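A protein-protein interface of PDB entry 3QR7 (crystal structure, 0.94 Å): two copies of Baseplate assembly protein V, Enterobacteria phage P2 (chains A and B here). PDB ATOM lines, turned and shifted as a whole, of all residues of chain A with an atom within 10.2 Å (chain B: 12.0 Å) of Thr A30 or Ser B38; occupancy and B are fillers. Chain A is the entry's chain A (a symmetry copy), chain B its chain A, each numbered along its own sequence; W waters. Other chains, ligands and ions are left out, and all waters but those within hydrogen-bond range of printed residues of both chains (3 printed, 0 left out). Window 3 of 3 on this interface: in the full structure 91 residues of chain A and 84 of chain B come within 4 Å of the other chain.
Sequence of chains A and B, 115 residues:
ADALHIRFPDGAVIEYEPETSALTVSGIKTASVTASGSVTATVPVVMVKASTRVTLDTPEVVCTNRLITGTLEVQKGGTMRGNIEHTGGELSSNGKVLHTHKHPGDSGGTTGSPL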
ATOM      1  N   ASP A  10     -35.409 -34.250  17.309  1.00  0.00           N
ATOM      2  CA  ASP A  10     -35.266 -34.381  18.737  1.00  0.00           C
ATOM      3  C   ASP A  10     -35.840 -33.183  19.506  1.00  0.00           C
ATOM      4  O   ASP A  10     -35.736 -33.155  20.726  1.00  0.00           O
ATOM      5  CB  ASP A  10     -33.824 -34.627  19.127  1.00  0.00           C
ATOM      6  CG  ASP A  10     -32.909 -33.452  18.808  1.00  0.00           C
ATOM      7  OD1 ASP A  10     -33.308 -32.565  18.032  1.00  0.00           O
ATOM      8  OD2 ASP A  10     -31.764 -33.478  19.344  1.00  0.00           O
ATOM      9  N   ALA A  12     -34.631 -30.093  19.065  1.00  0.00           N
ATOM     10  CA  ALA A  12     -33.644 -29.028  19.110  1.00  0.00           C
ATOM     11  C   ALA A  12     -33.984 -27.937  18.094  1.00  0.00           C
ATOM     12  O   ALA A  12     -34.613 -28.162  17.058  1.00  0.00           O
ATOM     13  CB  ALA A  12     -32.246 -29.564  18.845  1.00  0.00           C
ATOM     14  N   VAL A  13     -33.496 -26.741  18.413  1.00  0.00           N
ATOM     15  CA  VAL A  13     -33.585 -25.549  17.580  1.00  0.00           C
ATOM     16  C   VAL A  13     -32.159 -25.034  17.359  1.00  0.00           C
ATOM     17  O   VAL A  13     -31.416 -24.872  18.313  1.00  0.00           O
ATOM     18  CB  VAL A  13     -34.397 -24.443  18.311  1.00  0.00           C
ATOM     19  CG1 VAL A  13     -34.227 -23.087  17.654  1.00  0.00           C
ATOM     20  CG2 VAL A  13     -35.821 -24.879  18.460  1.00  0.00           C
ATOM     21  N   ILE A  14     -31.822 -24.725  16.107  1.00  0.00           N
ATOM     22  CA  ILE A  14     -30.646 -23.930  15.781  1.00  0.00           C
ATOM     23  C   ILE A  14     -31.124 -22.865  14.794  1.00  0.00           C
ATOM     24  O   ILE A  14     -31.582 -23.196  13.710  1.00  0.00           O
ATOM     25  CB  ILE A  14     -29.488 -24.735  15.196  1.00  0.00           C
ATOM     26  CG1 ILE A  14     -28.984 -25.743  16.228  1.00  0.00           C
ATOM     27  CG2 ILE A  14     -28.382 -23.802  14.718  1.00  0.00           C
ATOM     28  CD1 ILE A  14     -27.902 -26.688  15.726  1.00  0.00           C
ATOM     29  N   VAL A  25     -29.536 -21.693  20.133  1.00  0.00           N
ATOM     30  CA  VAL A  25     -29.349 -23.137  20.096  1.00  0.00           C
ATOM     31  C   VAL A  25     -30.059 -23.651  21.341  1.00  0.00           C
ATOM     32  O   VAL A  25     -29.729 -23.226  22.458  1.00  0.00           O
ATOM     33  CB  VAL A  25     -27.869 -23.524  20.106  1.00  0.00           C
ATOM     34  CG1 VAL A  25     -27.718 -25.043  20.223  1.00  0.00           C
ATOM     35  CG2 VAL A  25     -27.160 -22.984  18.885  1.00  0.00           C
ATOM     36  N   SER A  26     -31.042 -24.522  21.195  1.00  0.00           N
ATOM     37  CA  SER A  26     -31.764 -25.013  22.362  1.00  0.00           C
ATOM     38  C   SER A  26     -32.146 -26.463  22.154  1.00  0.00           C
ATOM     39  O   SER A  26     -32.177 -26.977  21.034  1.00  0.00           O
ATOM     40  CB  SER A  26     -33.006 -24.198  22.666  1.00  0.00           C
ATOM     41  OG  SER A  26     -33.960 -24.363  21.652  1.00  0.00           O
ATOM     42  N   GLY A  27     -32.467 -27.125  23.258  1.00  0.00           N
ATOM     43  CA  GLY A  27     -33.006 -28.477  23.191  1.00  0.00           C
ATOM     44  C   GLY A  27     -31.977 -29.530  22.823  1.00  0.00           C
ATOM     45  O   GLY A  27     -32.355 -30.622  22.396  1.00  0.00           O
ATOM     46  N   ILE A  28     -30.694 -29.224  23.000  1.00  0.00           N
ATOM     47  CA  ILE A  28     -29.621 -30.159  22.700  1.00  0.00           C
ATOM     48  C   ILE A  28     -29.170 -30.850  23.977  1.00  0.00           C
ATOM     49  O   ILE A  28     -29.511 -30.422  25.083  1.00  0.00           O
ATOM     50  CB  ILE A  28     -28.430 -29.460  21.984  1.00  0.00           C
ATOM     51  CG1 ILE A  28     -27.610 -28.616  22.946  1.00  0.00           C
ATOM     52  CG2 ILE A  28     -28.946 -28.634  20.802  1.00  0.00           C
ATOM     53  CD1 ILE A  28     -26.350 -28.017  22.295  1.00  0.00           C
ATOM     54  N   LYS A  29     -28.387 -31.932  23.850  1.00  0.00           N
ATOM     55  CA  LYS A  29     -27.720 -32.556  24.993  1.00  0.00           C
ATOM     56  C   LYS A  29     -26.265 -32.096  25.167  1.00  0.00           C
ATOM     57  O   LYS A  29     -25.827 -31.825  26.283  1.00  0.00           O
ATOM     58  CB  LYS A  29     -27.774 -34.080  24.893  1.00  0.00           C
ATOM     59  CG  LYS A  29     -29.171 -34.625  25.076  1.00  0.00           C
ATOM     60  CD  LYS A  29     -29.241 -36.142  24.766  1.00  0.00           C
ATOM     61  CE  LYS A  29     -30.640 -36.665  24.967  1.00  0.00           C
ATOM     62  NZ  LYS A  29     -30.767 -38.090  24.562  1.00  0.00           N
ATOM     63  N   THR A  30     -25.506 -32.051  24.064  1.00  0.00           N
ATOM     64  CA  THR A  30     -24.122 -31.654  24.151  1.00  0.00           C
ATOM     65  C   THR A  30     -23.776 -30.724  23.014  1.00  0.00           C
ATOM     66  O   THR A  30     -24.315 -30.816  21.910  1.00  0.00           O
ATOM     67  CB  THR A  30     -23.168 -32.869  24.115  1.00  0.00           C
ATOM     68  OG1 THR A  30     -23.332 -33.563  22.877  1.00  0.00           O
ATOM     69  CG2 THR A  30     -23.350 -33.760  25.293  1.00  0.00           C
ATOM     70  N   ALA A  31     -22.798 -29.852  23.282  1.00  0.00           N
ATOM     71  CA  ALA A  31     -22.131 -29.091  22.241  1.00  0.00           C
ATOM     72  C   ALA A  31     -20.636 -29.193  22.492  1.00  0.00           C
ATOM     73  O   ALA A  31     -20.193 -29.151  23.643  1.00  0.00           O
ATOM     74  CB  ALA A  31     -22.536 -27.630  22.217  1.00  0.00           C
ATOM     75  N   SER A  32     -19.858 -29.228  21.414  1.00  0.00           N
ATOM     76  CA  SER A  32     -18.459 -29.002  21.539  1.00  0.00           C
ATOM     77  C   SER A  32     -17.871 -28.297  20.388  1.00  0.00           C
ATOM     78  O   SER A  32     -18.344 -28.386  19.247  1.00  0.00           O
ATOM     79  CB  SER A  32     -17.735 -30.277  21.658  1.00  0.00           C
ATOM     80  OG  SER A  32     -17.720 -31.021  20.458  1.00  0.00           O
ATOM     81  N   VAL A  33     -16.842 -27.532  20.723  1.00  0.00           N
ATOM     82  CA  VAL A  33     -16.087 -26.759  19.768  1.00  0.00           C
ATOM     83  C   VAL A  33     -14.619 -27.111  19.972  1.00  0.00           C
ATOM     84  O   VAL A  33     -14.100 -26.927  21.064  1.00  0.00           O
ATOM     85  CB  VAL A  33     -16.351 -25.281  20.000  1.00  0.00           C
ATOM     86  CG1 VAL A  33     -15.555 -24.414  19.045  1.00  0.00           C
ATOM     87  CG2 VAL A  33     -17.865 -25.016  19.853  1.00  0.00           C
ATOM     88  N   VAL A  48     -23.048 -17.680  32.253  1.00  0.00           N
ATOM     89  CA  VAL A  48     -22.942 -19.125  32.226  1.00  0.00           C
ATOM     90  C   VAL A  48     -23.733 -19.640  33.414  1.00  0.00           C
ATOM     91  O   VAL A  48     -23.357 -19.396  34.565  1.00  0.00           O
ATOM     92  CB  VAL A  48     -21.494 -19.578  32.266  1.00  0.00           C
ATOM     93  CG1 VAL A  48     -21.424 -21.079  32.256  1.00  0.00           C
ATOM     94  CG2 VAL A  48     -20.702 -18.964  31.121  1.00  0.00           C
ATOM     95  N   LYS A  49     -24.813 -20.354  33.155  1.00  0.00           N
ATOM     96  CA  LYS A  49     -25.693 -20.891  34.190  1.00  0.00           C
ATOM     97  C   LYS A  49     -25.516 -22.408  34.154  1.00  0.00           C
ATOM     98  O   LYS A  49     -26.076 -23.072  33.281  1.00  0.00           O
ATOM     99  CB  LYS A  49     -27.141 -20.468  33.908  1.00  0.00           C
ATOM    100  CG  LYS A  49     -28.185 -20.876  34.921  1.00  0.00           C
ATOM    101  CD  LYS A  49     -27.942 -20.269  36.283  1.00  0.00           C
ATOM    102  CE  LYS A  49     -29.136 -20.428  37.206  1.00  0.00           C
ATOM    103  NZ  LYS A  49     -28.793 -20.038  38.614  1.00  0.00           N
ATOM    104  N   ALA A  50     -24.689 -22.918  35.053  1.00  0.00           N
ATOM    105  CA  ALA A  50     -24.230 -24.320  35.003  1.00  0.00           C
ATOM    106  C   ALA A  50     -24.544 -24.991  36.325  1.00  0.00           C
ATOM    107  O   ALA A  50     -23.869 -24.790  37.331  1.00  0.00           O
ATOM    108  CB  ALA A  50     -22.765 -24.426  34.669  1.00  0.00           C
ATOM    109  N   SER A  51     -25.580 -25.828  36.340  1.00  0.00           N
ATOM    110  CA  SER A  51     -26.073 -26.388  37.584  1.00  0.00           C
ATOM    111  C   SER A  51     -25.143 -27.375  38.260  1.00  0.00           C
ATOM    112  O   SER A  51     -25.362 -27.648  39.439  1.00  0.00           O
ATOM    113  CB  SER A  51     -27.455 -26.991  37.348  1.00  0.00           C
ATOM    114  OG  SER A  51     -27.395 -28.000  36.374  1.00  0.00           O
ATOM    115  N   THR A  52     -24.134 -27.891  37.566  1.00  0.00           N
ATOM    116  CA  THR A  52     -23.119 -28.734  38.181  1.00  0.00           C
ATOM    117  C   THR A  52     -21.768 -28.039  38.326  1.00  0.00           C
ATOM    118  O   THR A  52     -21.279 -27.923  39.447  1.00  0.00           O
ATOM    119  CB  THR A  52     -22.989 -30.104  37.439  1.00  0.00           C
ATOM    120  OG1 THR A  52     -24.189 -30.843  37.591  1.00  0.00           O
ATOM    121  CG2 THR A  52     -21.843 -30.922  37.977  1.00  0.00           C
ATOM    122  N   ARG A  53     -21.133 -27.581  37.241  1.00  0.00           N
ATOM    123  CA  ARG A  53     -19.749 -27.135  37.346  1.00  0.00           C
ATOM    124  C   ARG A  53     -19.325 -26.394  36.084  1.00  0.00           C
ATOM    125  O   ARG A  53     -19.768 -26.725  34.991  1.00  0.00           O
ATOM    126  CB  ARG A  53     -18.821 -28.337  37.549  1.00  0.00           C
ATOM    127  CG  ARG A  53     -17.376 -28.016  37.875  1.00  0.00           C
ATOM    128  CD  ARG A  53     -16.557 -29.277  38.173  1.00  0.00           C
ATOM    129  NE  ARG A  53     -17.099 -30.014  39.296  1.00  0.00           N
ATOM    130  CZ  ARG A  53     -17.915 -31.119  39.151  1.00  0.00           C
ATOM    131  NH1 ARG A  53     -18.560 -31.597  40.164  1.00  0.00           N
ATOM    132  NH2 ARG A  53     -18.060 -31.711  38.002  1.00  0.00           N
ATOM    133  N   VAL A  54     -18.403 -25.452  36.271  1.00  0.00           N
ATOM    134  CA  VAL A  54     -17.612 -24.866  35.206  1.00  0.00           C
ATOM    135  C   VAL A  54     -16.152 -25.160  35.488  1.00  0.00           C
ATOM    136  O   VAL A  54     -15.640 -24.784  36.529  1.00  0.00           O
ATOM    137  CB  VAL A  54     -17.820 -23.327  35.111  1.00  0.00           C
ATOM    138  CG1 VAL A  54     -16.907 -22.722  34.045  1.00  0.00           C
ATOM    139  CG2 VAL A  54     -19.268 -22.988  34.878  1.00  0.00           C
ATOM    140  N   THR A  55     -15.491 -25.857  34.555  1.00  0.00           N
ATOM    141  CA  THR A  55     -14.087 -26.177  34.680  1.00  0.00           C
ATOM    142  C   THR A  55     -13.285 -25.427  33.619  1.00  0.00           C
ATOM    143  O   THR A  55     -13.597 -25.523  32.424  1.00  0.00           O
ATOM    144  CB  THR A  55     -13.830 -27.694  34.547  1.00  0.00           C
ATOM    145  OG1 THR A  55     -14.523 -28.341  35.595  1.00  0.00           O
ATOM    146  CG2 THR A  55     -12.357 -28.021  34.646  1.00  0.00           C
ATOM    147  N   SER B  32     -27.619 -17.571  22.644  1.00  0.00           N
ATOM    148  CA  SER B  32     -27.693 -18.501  23.718  1.00  0.00           C
ATOM    149  C   SER B  32     -27.662 -19.906  23.284  1.00  0.00           C
ATOM    150  O   SER B  32     -28.088 -20.266  22.178  1.00  0.00           O
ATOM    151  CB  SER B  32     -28.943 -18.326  24.473  1.00  0.00           C
ATOM    152  OG  SER B  32     -30.085 -18.745  23.757  1.00  0.00           O
ATOM    153  N   VAL B  33     -27.087 -20.707  24.169  1.00  0.00           N
ATOM    154  CA  VAL B  33     -26.956 -22.131  23.981  1.00  0.00           C
ATOM    155  C   VAL B  33     -27.527 -22.799  25.226  1.00  0.00           C
ATOM    156  O   VAL B  33     -27.047 -22.542  26.322  1.00  0.00           O
ATOM    157  CB  VAL B  33     -25.492 -22.478  23.774  1.00  0.00           C
ATOM    158  CG1 VAL B  33     -25.289 -23.970  23.605  1.00  0.00           C
ATOM    159  CG2 VAL B  33     -24.966 -21.707  22.545  1.00  0.00           C
ATOM    160  N   THR B  34     -28.543 -23.656  25.053  1.00  0.00           N
ATOM    161  CA  THR B  34     -29.166 -24.383  26.162  1.00  0.00           C
ATOM    162  C   THR B  34     -29.064 -25.869  25.867  1.00  0.00           C
ATOM    163  O   THR B  34     -29.532 -26.331  24.824  1.00  0.00           O
ATOM    164  CB  THR B  34     -30.615 -23.961  26.353  1.00  0.00           C
ATOM    165  OG1 THR B  34     -30.642 -22.535  26.529  1.00  0.00           O
ATOM    166  CG2 THR B  34     -31.193 -24.624  27.573  1.00  0.00           C
ATOM    167  N   ALA B  35     -28.410 -26.584  26.782  1.00  0.00           N
ATOM    168  CA  ALA B  35     -28.086 -27.992  26.616  1.00  0.00           C
ATOM    169  C   ALA B  35     -28.372 -28.715  27.933  1.00  0.00           C
ATOM    170  O   ALA B  35     -28.203 -28.150  29.001  1.00  0.00           O
ATOM    171  CB  ALA B  35     -26.626 -28.152  26.242  1.00  0.00           C
ATOM    172  N   SER B  36     -28.730 -30.001  27.834  1.00  0.00           N
ATOM    173  CA  SER B  36     -29.048 -30.770  29.028  1.00  0.00           C
ATOM    174  C   SER B  36     -27.882 -31.528  29.634  1.00  0.00           C
ATOM    175  O   SER B  36     -28.005 -32.037  30.757  1.00  0.00           O
ATOM    176  CB  SER B  36     -30.189 -31.715  28.729  1.00  0.00           C
ATOM    177  OG  SER B  36     -29.804 -32.618  27.721  1.00  0.00           O
ATOM    178  N   GLY B  37     -26.762 -31.615  28.920  1.00  0.00           N
ATOM    179  CA  GLY B  37     -25.598 -32.397  29.327  1.00  0.00           C
ATOM    180  C   GLY B  37     -24.368 -31.541  29.563  1.00  0.00           C
ATOM    181  O   GLY B  37     -24.039 -31.185  30.702  1.00  0.00           O
ATOM    182  N   SER B  38     -23.678 -31.191  28.473  1.00  0.00           N
ATOM    183  CA  SER B  38     -22.410 -30.465  28.583  1.00  0.00           C
ATOM    184  C   SER B  38     -22.159 -29.588  27.386  1.00  0.00           C
ATOM    185  O   SER B  38     -22.599 -29.872  26.271  1.00  0.00           O
ATOM    186  CB  SER B  38     -21.245 -31.420  28.775  1.00  0.00           C
ATOM    187  OG  SER B  38     -21.092 -32.261  27.647  1.00  0.00           O
ATOM    188  N   VAL B  39     -21.379 -28.533  27.622  1.00  0.00           N
ATOM    189  CA  VAL B  39     -20.776 -27.692  26.583  1.00  0.00           C
ATOM    190  C   VAL B  39     -19.289 -27.693  26.826  1.00  0.00           C
ATOM    191  O   VAL B  39     -18.843 -27.403  27.935  1.00  0.00           O
ATOM    192  CB  VAL B  39     -21.339 -26.265  26.614  1.00  0.00           C
ATOM    193  CG1 VAL B  39     -20.589 -25.319  25.723  1.00  0.00           C
ATOM    194  CG2 VAL B  39     -22.831 -26.266  26.245  1.00  0.00           C
ATOM    195  N   THR B  40     -18.533 -28.020  25.774  1.00  0.00           N
ATOM    196  CA  THR B  40     -17.086 -28.165  25.845  1.00  0.00           C
ATOM    197  C   THR B  40     -16.418 -27.331  24.775  1.00  0.00           C
ATOM    198  O   THR B  40     -16.881 -27.304  23.626  1.00  0.00           O
ATOM    199  CB  THR B  40     -16.687 -29.622  25.681  1.00  0.00           C
ATOM    200  OG1 THR B  40     -17.389 -30.412  26.642  1.00  0.00           O
ATOM    201  CG2 THR B  40     -15.204 -29.850  25.844  1.00  0.00           C
ATOM    202  N   ALA B  41     -15.335 -26.668  25.142  1.00  0.00           N
ATOM    203  CA  ALA B  41     -14.479 -25.966  24.190  1.00  0.00           C
ATOM    204  C   ALA B  41     -13.046 -26.415  24.442  1.00  0.00           C
ATOM    205  O   ALA B  41     -12.595 -26.349  25.574  1.00  0.00           O
ATOM    206  CB  ALA B  41     -14.576 -24.453  24.342  1.00  0.00           C
ATOM    207  N   THR B  42     -12.377 -26.845  23.374  1.00  0.00           N
ATOM    208  CA  THR B  42     -10.999 -27.358  23.447  1.00  0.00           C
ATOM    209  C   THR B  42     -10.170 -26.625  22.427  1.00  0.00           C
ATOM    210  O   THR B  42     -10.367 -26.812  21.231  1.00  0.00           O
ATOM    211  CB  THR B  42     -10.993 -28.867  23.181  1.00  0.00           C
ATOM    212  OG1 THR B  42     -11.908 -29.501  24.052  1.00  0.00           O
ATOM    213  CG2 THR B  42      -9.613 -29.428  23.368  1.00  0.00           C
ATOM    214  N   THR B  58     -22.858 -21.091  39.127  1.00  0.00           N
ATOM    215  CA  THR B  58     -22.625 -22.515  39.206  1.00  0.00           C
ATOM    216  C   THR B  58     -22.248 -22.861  40.633  1.00  0.00           C
ATOM    217  O   THR B  58     -21.648 -22.040  41.333  1.00  0.00           O
ATOM    218  CB  THR B  58     -21.478 -22.918  38.226  1.00  0.00           C
ATOM    219  OG1 THR B  58     -21.306 -24.312  38.213  1.00  0.00           O
ATOM    220  CG2 THR B  58     -20.170 -22.271  38.519  1.00  0.00           C
HETATM  221  O   HOH W   1     -19.758 -31.284  25.450  1.00  0.00           O
HETATM  222  O   HOH W   2     -31.045 -21.298  24.107  1.00  0.00           O
HETATM  223  O   HOH W   3     -14.191 -29.618  22.602  1.00  0.00           O
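O of Ser B32 is in hydrogen-bond range of N of Val A25, at 2.9 Å. The backbone carbonyl oxygen of Val A25 lies within hydrogen-bond range of the backbone NH of Thr B34, at 2.9 Å. O of Thr B34 is in hydrogen-bond range of N of Gly A27. The backbone carbonyl oxygen (O) of Ile A28 lies within hydrogen-bond range of the backbone NH (N) of Ser B36 (2.9 Å). The backbone NH (N) of Gly B37 sits at hydrogen-bond distance from the backbone carbonyl oxygen (O) of Lys A29, at 2.8 Å. N of Ser B38 lies within hydrogen-bond range of O of Lys A29 (3.1 Å). O of Ser B38 lies within hydrogen-bond range of N of Ala A31, at 3.0 Å. N of Thr B40 is in hydrogen-bond range of O of Ala A31, 2.9 Å away. O of Thr B40 sits at hydrogen-bond distance from N of Val A33, 2.9 Å away. The backbone NH of Thr B42 is in hydrogen-bond range of the backbone carbonyl oxygen of Val A33 (2.9 Å). The side-chain hydroxyl (OG1) of Thr B58 is in hydrogen-bond range of the backbone carbonyl oxygen (O) of Ala A50. The side-chain hydroxyl of Thr B58 sits close to the backbone NH of Arg A53 (3.4 Å).
N of Ser A26 sits at hydrogen-bond distance from O of Val A13.
Val A25 touches Val B33. O of Thr B34 touches CA of Ser A26, at 3.6 Å. Ile A28 touches Ala B35 (O to CA, 3.2 Å). Ala B35 touches Lys A29 (CB to O, 3.8 Å). Ser B36 touches Lys A29. Ser B38 touches Thr A30 (O to CA, 3.2 Å). Ala A31 touches Val B39. Ser A32 touches Thr B40 (CA to O, 3.1 Å). Thr B58 touches Thr A52 (OG1 to C, 3.8 Å). Val A54 touches Thr B58 (N to OG1, 3.7 Å).
Of the printed residues of chain A, Ser B38 touches Lys A29 (3.1 Å), Thr A30 (3.2 Å) and Ala A31 (3.0 Å). Of the printed residues of chain B, Ala A31 touches Ser B38 (3.0 Å), Val B39 (3.3 Å) and Thr B40 (2.9 Å). Val B39 touches just one residue of chain A: Ala A31 (3.3 Å). Of the printed residues of chain A, Thr B42 touches Val A33 (2.9 Å). Printed residues of chain A within 4 Å of Ser B32: Val A25. Printed residues of chain B within 4 Å of Arg A53: Thr B58 (3.3 Å). Ala A12 touches none of the printed residues of chain B. The nearest printed residue of chain A that does not touch Ser B38 is Ser A32 (5.6 Å).
Hydrophobic or aromatic side chains of chain A that line the printed part of chain B: Val A25, Ile A28, Ala A50 and Val A54. Of the 12 printed residues of chain B, 12 touch a printed residue of chain A. Among the printed residues, 24 pairs touch across the chains. Among the printed residues, no Asp or Glu carboxylate lies within 4 Å of a Lys or Arg side-chain nitrogen of the other chain.
Positions printed for both chains: 32 and 33.
Water W3 lies within hydrogen-bond range of the side-chain hydroxyl of Thr B42 (2.7 Å) and the backbone carbonyl oxygen of Val A33 (3.1 Å). Water W2 lies within hydrogen-bond range of the side-chain hydroxyl (OG1) of Thr B34, the side-chain hydroxyl (OG) of Ser B32 and the backbone carbonyl oxygen (O) of Val A25. Water W1 lies within hydrogen-bond range of OG of Ser B38 (2.7 Å), OG1 of Thr B40 (2.8 Å) and O of Ala A31 (2.8 Å).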
